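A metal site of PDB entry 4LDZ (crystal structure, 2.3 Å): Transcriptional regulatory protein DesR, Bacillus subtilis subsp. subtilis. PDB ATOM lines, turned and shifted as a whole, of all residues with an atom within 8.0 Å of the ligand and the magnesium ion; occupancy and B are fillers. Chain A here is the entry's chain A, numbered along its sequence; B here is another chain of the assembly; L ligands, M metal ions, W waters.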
ATOM      1  N   ALA A  11      15.714 -26.647 -24.970  1.00  0.00           N
ATOM      2  CA  ALA A  11      16.267 -25.376 -24.452  1.00  0.00           C
ATOM      3  C   ALA A  11      16.959 -25.725 -23.117  1.00  0.00           C
ATOM      4  O   ALA A  11      16.301 -26.194 -22.177  1.00  0.00           O
ATOM      5  CB  ALA A  11      15.163 -24.337 -24.272  1.00  0.00           C
ATOM      6  N   GLU A  12      18.310 -25.655 -23.101  1.00  0.00           N
ATOM      7  CA  GLU A  12      19.158 -26.010 -21.966  1.00  0.00           C
ATOM      8  C   GLU A  12      20.456 -25.214 -22.010  1.00  0.00           C
ATOM      9  O   GLU A  12      21.169 -25.260 -23.012  1.00  0.00           O
ATOM     10  CB  GLU A  12      19.407 -27.541 -21.957  1.00  0.00           C
ATOM     11  CG  GLU A  12      20.413 -28.042 -20.947  1.00  0.00           C
ATOM     12  CD  GLU A  12      20.122 -27.643 -19.505  1.00  0.00           C
ATOM     13  OE1 GLU A  12      19.000 -27.914 -19.030  1.00  0.00           O
ATOM     14  OE2 GLU A  12      21.016 -27.052 -18.865  1.00  0.00           O
ATOM     15  N   ASP A  13      20.739 -24.408 -20.975  1.00  0.00           N
ATOM     16  CA  ASP A  13      21.938 -23.566 -20.985  1.00  0.00           C
ATOM     17  C   ASP A  13      23.241 -24.314 -20.756  1.00  0.00           C
ATOM     18  O   ASP A  13      24.299 -23.804 -21.101  1.00  0.00           O
ATOM     19  CB  ASP A  13      21.816 -22.348 -20.056  1.00  0.00           C
ATOM     20  CG  ASP A  13      21.657 -22.632 -18.575  1.00  0.00           C
ATOM     21  OD1 ASP A  13      21.085 -23.682 -18.236  1.00  0.00           O
ATOM     22  OD2 ASP A  13      22.043 -21.764 -17.759  1.00  0.00           O
ATOM     23  N   GLN A  14      23.185 -25.510 -20.173  1.00  0.00           N
ATOM     24  CA  GLN A  14      24.391 -26.300 -19.910  1.00  0.00           C
ATOM     25  C   GLN A  14      24.661 -27.125 -21.179  1.00  0.00           C
ATOM     26  O   GLN A  14      23.947 -28.053 -21.463  1.00  0.00           O
ATOM     27  CB  GLN A  14      24.168 -27.165 -18.670  1.00  0.00           C
ATOM     28  CG  GLN A  14      25.446 -27.763 -18.106  1.00  0.00           C
ATOM     29  CD  GLN A  14      25.125 -28.767 -17.033  1.00  0.00           C
ATOM     30  OE1 GLN A  14      25.303 -28.488 -15.849  1.00  0.00           O
ATOM     31  NE2 GLN A  14      24.608 -29.929 -17.410  1.00  0.00           N
ATOM     32  N   LEU A  17      24.786 -31.060 -21.136  1.00  0.00           N
ATOM     33  CA  LEU A  17      23.495 -31.723 -21.050  1.00  0.00           C
ATOM     34  C   LEU A  17      22.667 -31.553 -22.304  1.00  0.00           C
ATOM     35  O   LEU A  17      22.068 -32.546 -22.756  1.00  0.00           O
ATOM     36  CB  LEU A  17      22.710 -31.303 -19.804  1.00  0.00           C
ATOM     37  CG  LEU A  17      21.360 -31.993 -19.551  1.00  0.00           C
ATOM     38  CD1 LEU A  17      21.496 -33.536 -19.395  1.00  0.00           C
ATOM     39  CD2 LEU A  17      20.721 -31.406 -18.354  1.00  0.00           C
ATOM     40  N   THR A  38      19.997 -22.424 -25.998  1.00  0.00           N
ATOM     41  CA  THR A  38      20.578 -22.226 -24.669  1.00  0.00           C
ATOM     42  C   THR A  38      19.874 -21.193 -23.813  1.00  0.00           C
ATOM     43  O   THR A  38      20.268 -20.996 -22.656  1.00  0.00           O
ATOM     44  CB  THR A  38      22.101 -21.952 -24.779  1.00  0.00           C
ATOM     45  OG1 THR A  38      22.312 -20.927 -25.751  1.00  0.00           O
ATOM     46  CG2 THR A  38      22.906 -23.201 -25.164  1.00  0.00           C
ATOM     47  N   MET A  57      12.237 -27.993 -21.858  1.00  0.00           N
ATOM     48  CA  MET A  57      12.589 -26.685 -21.391  1.00  0.00           C
ATOM     49  C   MET A  57      13.248 -26.629 -20.018  1.00  0.00           C
ATOM     50  O   MET A  57      12.619 -26.999 -19.025  1.00  0.00           O
ATOM     51  CB  MET A  57      11.296 -25.859 -21.395  1.00  0.00           C
ATOM     52  CG  MET A  57      11.505 -24.406 -21.154  1.00  0.00           C
ATOM     53  SD  MET A  57      11.825 -23.431 -22.632  1.00  0.00           S
ATOM     54  CE  MET A  57      10.202 -23.295 -23.237  1.00  0.00           C
ATOM     55  N   ASP A  58      14.486 -26.108 -19.942  1.00  0.00           N
ATOM     56  CA  ASP A  58      15.188 -25.870 -18.684  1.00  0.00           C
ATOM     57  C   ASP A  58      14.561 -24.587 -18.089  1.00  0.00           C
ATOM     58  O   ASP A  58      14.057 -23.769 -18.857  1.00  0.00           O
ATOM     59  CB  ASP A  58      16.674 -25.591 -18.953  1.00  0.00           C
ATOM     60  CG  ASP A  58      17.512 -25.352 -17.703  1.00  0.00           C
ATOM     61  OD1 ASP A  58      17.174 -25.917 -16.628  1.00  0.00           O
ATOM     62  OD2 ASP A  58      18.503 -24.602 -17.797  1.00  0.00           O
ATOM     63  N   ILE A  59      14.588 -24.377 -16.764  1.00  0.00           N
ATOM     64  CA  ILE A  59      14.070 -23.126 -16.189  1.00  0.00           C
ATOM     65  C   ILE A  59      15.164 -22.065 -16.224  1.00  0.00           C
ATOM     66  O   ILE A  59      15.020 -21.074 -16.935  1.00  0.00           O
ATOM     67  CB  ILE A  59      13.458 -23.280 -14.787  1.00  0.00           C
ATOM     68  CG1 ILE A  59      12.222 -24.179 -14.821  1.00  0.00           C
ATOM     69  CG2 ILE A  59      13.154 -21.875 -14.208  1.00  0.00           C
ATOM     70  CD1 ILE A  59      11.615 -24.472 -13.459  1.00  0.00           C
ATOM     71  N   GLU A  60      16.227 -22.241 -15.428  1.00  0.00           N
ATOM     72  CA  GLU A  60      17.315 -21.283 -15.330  1.00  0.00           C
ATOM     73  C   GLU A  60      18.242 -21.277 -16.537  1.00  0.00           C
ATOM     74  O   GLU A  60      18.987 -22.230 -16.806  1.00  0.00           O
ATOM     75  CB  GLU A  60      18.067 -21.426 -14.007  1.00  0.00           C
ATOM     76  CG  GLU A  60      17.206 -21.046 -12.814  1.00  0.00           C
ATOM     77  CD  GLU A  60      17.864 -21.107 -11.444  1.00  0.00           C
ATOM     78  OE1 GLU A  60      17.124 -21.163 -10.444  1.00  0.00           O
ATOM     79  OE2 GLU A  60      19.120 -21.109 -11.363  1.00  0.00           O
ATOM     80  N   MET A  61      18.107 -20.211 -17.313  1.00  0.00           N
ATOM     81  CA  MET A  61      18.877 -19.969 -18.528  1.00  0.00           C
ATOM     82  C   MET A  61      19.074 -18.469 -18.611  1.00  0.00           C
ATOM     83  O   MET A  61      18.196 -17.745 -18.165  1.00  0.00           O
ATOM     84  CB  MET A  61      18.101 -20.441 -19.767  1.00  0.00           C
ATOM     85  CG  MET A  61      17.752 -21.885 -19.775  1.00  0.00           C
ATOM     86  SD  MET A  61      17.092 -22.312 -21.379  1.00  0.00           S
ATOM     87  CE  MET A  61      15.345 -21.929 -21.139  1.00  0.00           C
ATOM     88  N   PRO A  62      20.179 -17.977 -19.238  1.00  0.00           N
ATOM     89  CA  PRO A  62      20.346 -16.513 -19.355  1.00  0.00           C
ATOM     90  C   PRO A  62      19.382 -15.862 -20.337  1.00  0.00           C
ATOM     91  O   PRO A  62      18.863 -16.533 -21.233  1.00  0.00           O
ATOM     92  CB  PRO A  62      21.806 -16.346 -19.813  1.00  0.00           C
ATOM     93  CG  PRO A  62      22.251 -17.646 -20.302  1.00  0.00           C
ATOM     94  CD  PRO A  62      21.317 -18.722 -19.817  1.00  0.00           C
ATOM     95  N   THR A  65      14.097 -16.970 -18.936  1.00  0.00           N
ATOM     96  CA  THR A  65      13.968 -18.288 -18.301  1.00  0.00           C
ATOM     97  C   THR A  65      13.040 -19.194 -19.124  1.00  0.00           C
ATOM     98  O   THR A  65      12.360 -18.726 -20.042  1.00  0.00           O
ATOM     99  CB  THR A  65      13.472 -18.131 -16.827  1.00  0.00           C
ATOM    100  OG1 THR A  65      12.080 -17.829 -16.793  1.00  0.00           O
ATOM    101  CG2 THR A  65      14.266 -17.099 -16.036  1.00  0.00           C
ATOM    102  N   GLY A  66      12.980 -20.458 -18.773  1.00  0.00           N
ATOM    103  CA  GLY A  66      12.081 -21.417 -19.390  1.00  0.00           C
ATOM    104  C   GLY A  66      10.646 -21.147 -18.979  1.00  0.00           C
ATOM    105  O   GLY A  66       9.721 -21.527 -19.703  1.00  0.00           O
ATOM    106  N   LEU A  67      10.454 -20.481 -17.824  1.00  0.00           N
ATOM    107  CA  LEU A  67       9.115 -20.143 -17.331  1.00  0.00           C
ATOM    108  C   LEU A  67       8.531 -18.942 -18.067  1.00  0.00           C
ATOM    109  O   LEU A  67       7.358 -18.980 -18.430  1.00  0.00           O
ATOM    110  CB  LEU A  67       9.055 -19.977 -15.790  1.00  0.00           C
ATOM    111  CG  LEU A  67       9.392 -21.230 -14.944  1.00  0.00           C
ATOM    112  CD1 LEU A  67       9.469 -20.879 -13.476  1.00  0.00           C
ATOM    113  CD2 LEU A  67       8.359 -22.338 -15.112  1.00  0.00           C
ATOM    114  N   ILE A  82       8.882 -29.048 -18.806  1.00  0.00           N
ATOM    115  CA  ILE A  82       9.950 -28.457 -18.005  1.00  0.00           C
ATOM    116  C   ILE A  82      10.890 -29.610 -17.551  1.00  0.00           C
ATOM    117  O   ILE A  82      10.402 -30.638 -17.097  1.00  0.00           O
ATOM    118  CB  ILE A  82       9.357 -27.716 -16.758  1.00  0.00           C
ATOM    119  CG1 ILE A  82       8.525 -26.468 -17.137  1.00  0.00           C
ATOM    120  CG2 ILE A  82      10.440 -27.400 -15.695  1.00  0.00           C
ATOM    121  CD1 ILE A  82       9.220 -25.374 -18.000  1.00  0.00           C
ATOM    122  N   LEU A  83      12.207 -29.436 -17.702  1.00  0.00           N
ATOM    123  CA  LEU A  83      13.231 -30.406 -17.233  1.00  0.00           C
ATOM    124  C   LEU A  83      14.229 -29.565 -16.455  1.00  0.00           C
ATOM    125  O   LEU A  83      14.948 -28.781 -17.055  1.00  0.00           O
ATOM    126  CB  LEU A  83      13.906 -31.199 -18.362  1.00  0.00           C
ATOM    127  CG  LEU A  83      14.999 -32.197 -17.902  1.00  0.00           C
ATOM    128  CD1 LEU A  83      14.435 -33.263 -16.944  1.00  0.00           C
ATOM    129  CD2 LEU A  83      15.666 -32.834 -19.078  1.00  0.00           C
ATOM    130  N   THR A  84      14.204 -29.646 -15.133  1.00  0.00           N
ATOM    131  CA  THR A  84      15.007 -28.733 -14.297  1.00  0.00           C
ATOM    132  C   THR A  84      15.687 -29.420 -13.118  1.00  0.00           C
ATOM    133  O   THR A  84      15.275 -30.508 -12.724  1.00  0.00           O
ATOM    134  CB  THR A  84      14.059 -27.580 -13.814  1.00  0.00           C
ATOM    135  OG1 THR A  84      14.780 -26.603 -13.078  1.00  0.00           O
ATOM    136  CG2 THR A  84      12.913 -28.079 -12.961  1.00  0.00           C
ATOM    137  N   THR A  85      16.690 -28.765 -12.526  1.00  0.00           N
ATOM    138  CA  THR A  85      17.370 -29.216 -11.316  1.00  0.00           C
ATOM    139  C   THR A  85      16.477 -28.894 -10.094  1.00  0.00           C
ATOM    140  O   THR A  85      16.468 -29.634  -9.122  1.00  0.00           O
ATOM    141  CB  THR A  85      18.708 -28.470 -11.194  1.00  0.00           C
ATOM    142  OG1 THR A  85      19.525 -28.785 -12.320  1.00  0.00           O
ATOM    143  CG2 THR A  85      19.474 -28.797  -9.927  1.00  0.00           C
ATOM    144  N   PHE A  86      15.718 -27.791 -10.182  1.00  0.00           N
ATOM    145  CA  PHE A  86      14.922 -27.143  -9.141  1.00  0.00           C
ATOM    146  C   PHE A  86      13.514 -27.585  -8.860  1.00  0.00           C
ATOM    147  O   PHE A  86      12.606 -27.372  -9.677  1.00  0.00           O
ATOM    148  CB  PHE A  86      14.971 -25.602  -9.317  1.00  0.00           C
ATOM    149  CG  PHE A  86      16.347 -25.134  -9.711  1.00  0.00           C
ATOM    150  CD1 PHE A  86      17.388 -25.107  -8.787  1.00  0.00           C
ATOM    151  CD2 PHE A  86      16.642 -24.833 -11.040  1.00  0.00           C
ATOM    152  CE1 PHE A  86      18.674 -24.728  -9.163  1.00  0.00           C
ATOM    153  CE2 PHE A  86      17.931 -24.467 -11.419  1.00  0.00           C
ATOM    154  CZ  PHE A  86      18.932 -24.399 -10.485  1.00  0.00           C
ATOM    155  N   TYR A  91       8.538 -22.155  -8.684  1.00  0.00           N
ATOM    156  CA  TYR A  91       8.792 -22.630 -10.047  1.00  0.00           C
ATOM    157  C   TYR A  91       7.643 -23.550 -10.509  1.00  0.00           C
ATOM    158  O   TYR A  91       7.062 -23.293 -11.555  1.00  0.00           O
ATOM    159  CB  TYR A  91      10.144 -23.340 -10.115  1.00  0.00           C
ATOM    160  CG  TYR A  91      11.375 -22.440 -10.191  1.00  0.00           C
ATOM    161  CD1 TYR A  91      11.249 -21.057 -10.249  1.00  0.00           C
ATOM    162  CD2 TYR A  91      12.647 -22.989 -10.292  1.00  0.00           C
ATOM    163  CE1 TYR A  91      12.384 -20.236 -10.327  1.00  0.00           C
ATOM    164  CE2 TYR A  91      13.785 -22.181 -10.372  1.00  0.00           C
ATOM    165  CZ  TYR A  91      13.653 -20.803 -10.415  1.00  0.00           C
ATOM    166  OH  TYR A  91      14.769 -20.008 -10.558  1.00  0.00           O
ATOM    167  N   TYR A 103       6.489 -31.624 -16.033  1.00  0.00           N
ATOM    168  CA  TYR A 103       7.423 -31.014 -15.104  1.00  0.00           C
ATOM    169  C   TYR A 103       8.225 -32.116 -14.508  1.00  0.00           C
ATOM    170  O   TYR A 103       7.740 -32.908 -13.682  1.00  0.00           O
ATOM    171  CB  TYR A 103       6.750 -30.098 -14.059  1.00  0.00           C
ATOM    172  CG  TYR A 103       7.696 -29.131 -13.365  1.00  0.00           C
ATOM    173  CD1 TYR A 103       8.681 -29.597 -12.499  1.00  0.00           C
ATOM    174  CD2 TYR A 103       7.563 -27.759 -13.512  1.00  0.00           C
ATOM    175  CE1 TYR A 103       9.494 -28.719 -11.797  1.00  0.00           C
ATOM    176  CE2 TYR A 103       8.400 -26.872 -12.830  1.00  0.00           C
ATOM    177  CZ  TYR A 103       9.351 -27.355 -11.951  1.00  0.00           C
ATOM    178  OH  TYR A 103      10.172 -26.518 -11.258  1.00  0.00           O
ATOM    179  N   LEU A 104       9.438 -32.214 -15.001  1.00  0.00           N
ATOM    180  CA  LEU A 104      10.389 -33.248 -14.642  1.00  0.00           C
ATOM    181  C   LEU A 104      11.603 -32.691 -13.983  1.00  0.00           C
ATOM    182  O   LEU A 104      12.004 -31.538 -14.215  1.00  0.00           O
ATOM    183  CB  LEU A 104      10.794 -33.984 -15.919  1.00  0.00           C
ATOM    184  CG  LEU A 104       9.687 -34.693 -16.698  1.00  0.00           C
ATOM    185  CD1 LEU A 104      10.293 -35.475 -17.844  1.00  0.00           C
ATOM    186  CD2 LEU A 104       8.934 -35.645 -15.797  1.00  0.00           C
ATOM    187  N   LEU A 105      12.213 -33.538 -13.152  1.00  0.00           N
ATOM    188  CA  LEU A 105      13.421 -33.226 -12.421  1.00  0.00           C
ATOM    189  C   LEU A 105      14.619 -33.944 -13.033  1.00  0.00           C
ATOM    190  O   LEU A 105      14.487 -35.072 -13.538  1.00  0.00           O
ATOM    191  CB  LEU A 105      13.254 -33.533 -10.912  1.00  0.00           C
ATOM    192  CG  LEU A 105      12.132 -32.690 -10.195  1.00  0.00           C
ATOM    193  CD1 LEU A 105      11.827 -33.216  -8.797  1.00  0.00           C
ATOM    194  CD2 LEU A 105      12.520 -31.229 -10.091  1.00  0.00           C
ATOM    195  N   LYS A 106      15.793 -33.275 -13.020  1.00  0.00           N
ATOM    196  CA  LYS A 106      17.051 -33.790 -13.557  1.00  0.00           C
ATOM    197  C   LYS A 106      17.614 -34.943 -12.719  1.00  0.00           C
ATOM    198  O   LYS A 106      18.545 -35.635 -13.129  1.00  0.00           O
ATOM    199  CB  LYS A 106      18.059 -32.652 -13.785  1.00  0.00           C
ATOM    200  CG  LYS A 106      17.744 -31.794 -15.028  1.00  0.00           C
ATOM    201  CD  LYS A 106      18.710 -30.600 -15.147  1.00  0.00           C
ATOM    202  CE  LYS A 106      18.405 -29.749 -16.350  1.00  0.00           C
ATOM    203  NZ  LYS A 106      19.225 -28.506 -16.361  1.00  0.00           N
ATOM    204  N   GLN B  14      23.475 -36.060 -10.650  1.00  0.00           N
ATOM    205  CA  GLN B  14      22.286 -35.701 -11.418  1.00  0.00           C
ATOM    206  C   GLN B  14      22.025 -36.858 -12.382  1.00  0.00           C
ATOM    207  O   GLN B  14      22.742 -37.026 -13.361  1.00  0.00           O
ATOM    208  CB  GLN B  14      22.532 -34.372 -12.128  1.00  0.00           C
ATOM    209  CG  GLN B  14      21.293 -33.699 -12.624  1.00  0.00           C
ATOM    210  CD  GLN B  14      21.648 -32.497 -13.458  1.00  0.00           C
ATOM    211  OE1 GLN B  14      21.573 -31.349 -13.005  1.00  0.00           O
ATOM    212  NE2 GLN B  14      22.099 -32.748 -14.682  1.00  0.00           N
HETATM  213 BE1  LIG L   1      17.528 -25.509 -15.225  1.00  0.00          BE
HETATM  214  F1  LIG L   1      16.249 -24.789 -14.367  1.00  0.00           F
HETATM  215  F2  LIG L   1      17.932 -26.903 -14.384  1.00  0.00           F
HETATM  216  F3  LIG L   1      18.858 -24.501 -15.028  1.00  0.00           F
HETATM  217 MG    MG M   1      19.953 -24.075 -16.509  1.00  0.00          MG
HETATM  218  O   HOH W   1      21.407 -23.538 -15.192  1.00  0.00           O
HETATM  219  O   HOH W   2      21.007 -25.920 -16.800  1.00  0.00           O
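The side-chain carboxylate (OD1) of Asp 58 binds a beryllium atom (BE1) of the ligand, at 1.5 Å. N of Glu 60 lies within hydrogen-bond range of F1 of the ligand (2.8 Å). The side-chain hydroxyl (OG1) of Thr 84 lies within hydrogen-bond range of a fluorine (F1) of the ligand (2.7 Å). A fluorine (F2) of the ligand lies within hydrogen-bond range of the side-chain amino group (NZ) of Lys 106 (2.9 Å). The backbone NH of Thr 85 is in hydrogen-bond range of a fluorine (F2) of the ligand (2.9 Å). The side-chain hydroxyl (OG1) of Thr 85 lies within hydrogen-bond range of a fluorine (F2) of the ligand. N of Ile 59 is in hydrogen-bond range of F1 of the ligand.
NZ of Lys 106 sits close to OD1 of Asp 58. The backbone carbonyl oxygen of Asp 58 sits close to the backbone NH of Gly 66 (3.5 Å). The backbone carbonyl oxygen of Ala 11 lies within hydrogen-bond range of the backbone NH of Asp 58 (2.9 Å). The backbone NH of Phe 86 sits at hydrogen-bond distance from the side-chain hydroxyl of Thr 84 (3.3 Å). O of Leu 104 is in hydrogen-bond range of N of Thr 84, 3.0 Å away. The side-chain amino group (NZ) of Lys 106 is in salt-bridge range of the side-chain carboxylate (OE1) of Glu 12, at 2.7 Å. The backbone NH (N) of Gly 66 sits at hydrogen-bond distance from the backbone carbonyl oxygen (O) of Ile 59, 2.8 Å away. N of Gln 14 of chain A sits at hydrogen-bond distance from OE2 of Glu 12, 3.0 Å away.
Residues that only touch the ligand: Phe 86. Hydrophobic or aromatic side chains within 4 Å of the ligand: Ile 59 and Phe 86. Of the 26 residues printed, 8 come within 4 Å of the ligand. The nearest printed residue that does not touch the ligand is Leu 83 (4.4 Å).
Residues that only touch the magnesium ion: Glu 12. Four residues have an atom within 4 Å of the magnesium ion: Glu 12, Asp 13, Asp 58 and Glu 60. The nearest printed residue that does not touch the magnesium ion is Met 61 (4.4 Å).
The magnesium ion is bound by a fluorine (F3) of the ligand, the side-chain carboxylate (OD2) of Asp 58, water W1, the side-chain carboxylate (OD1) of Asp 13, the backbone carbonyl oxygen (O) of Glu 60 and water W2.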
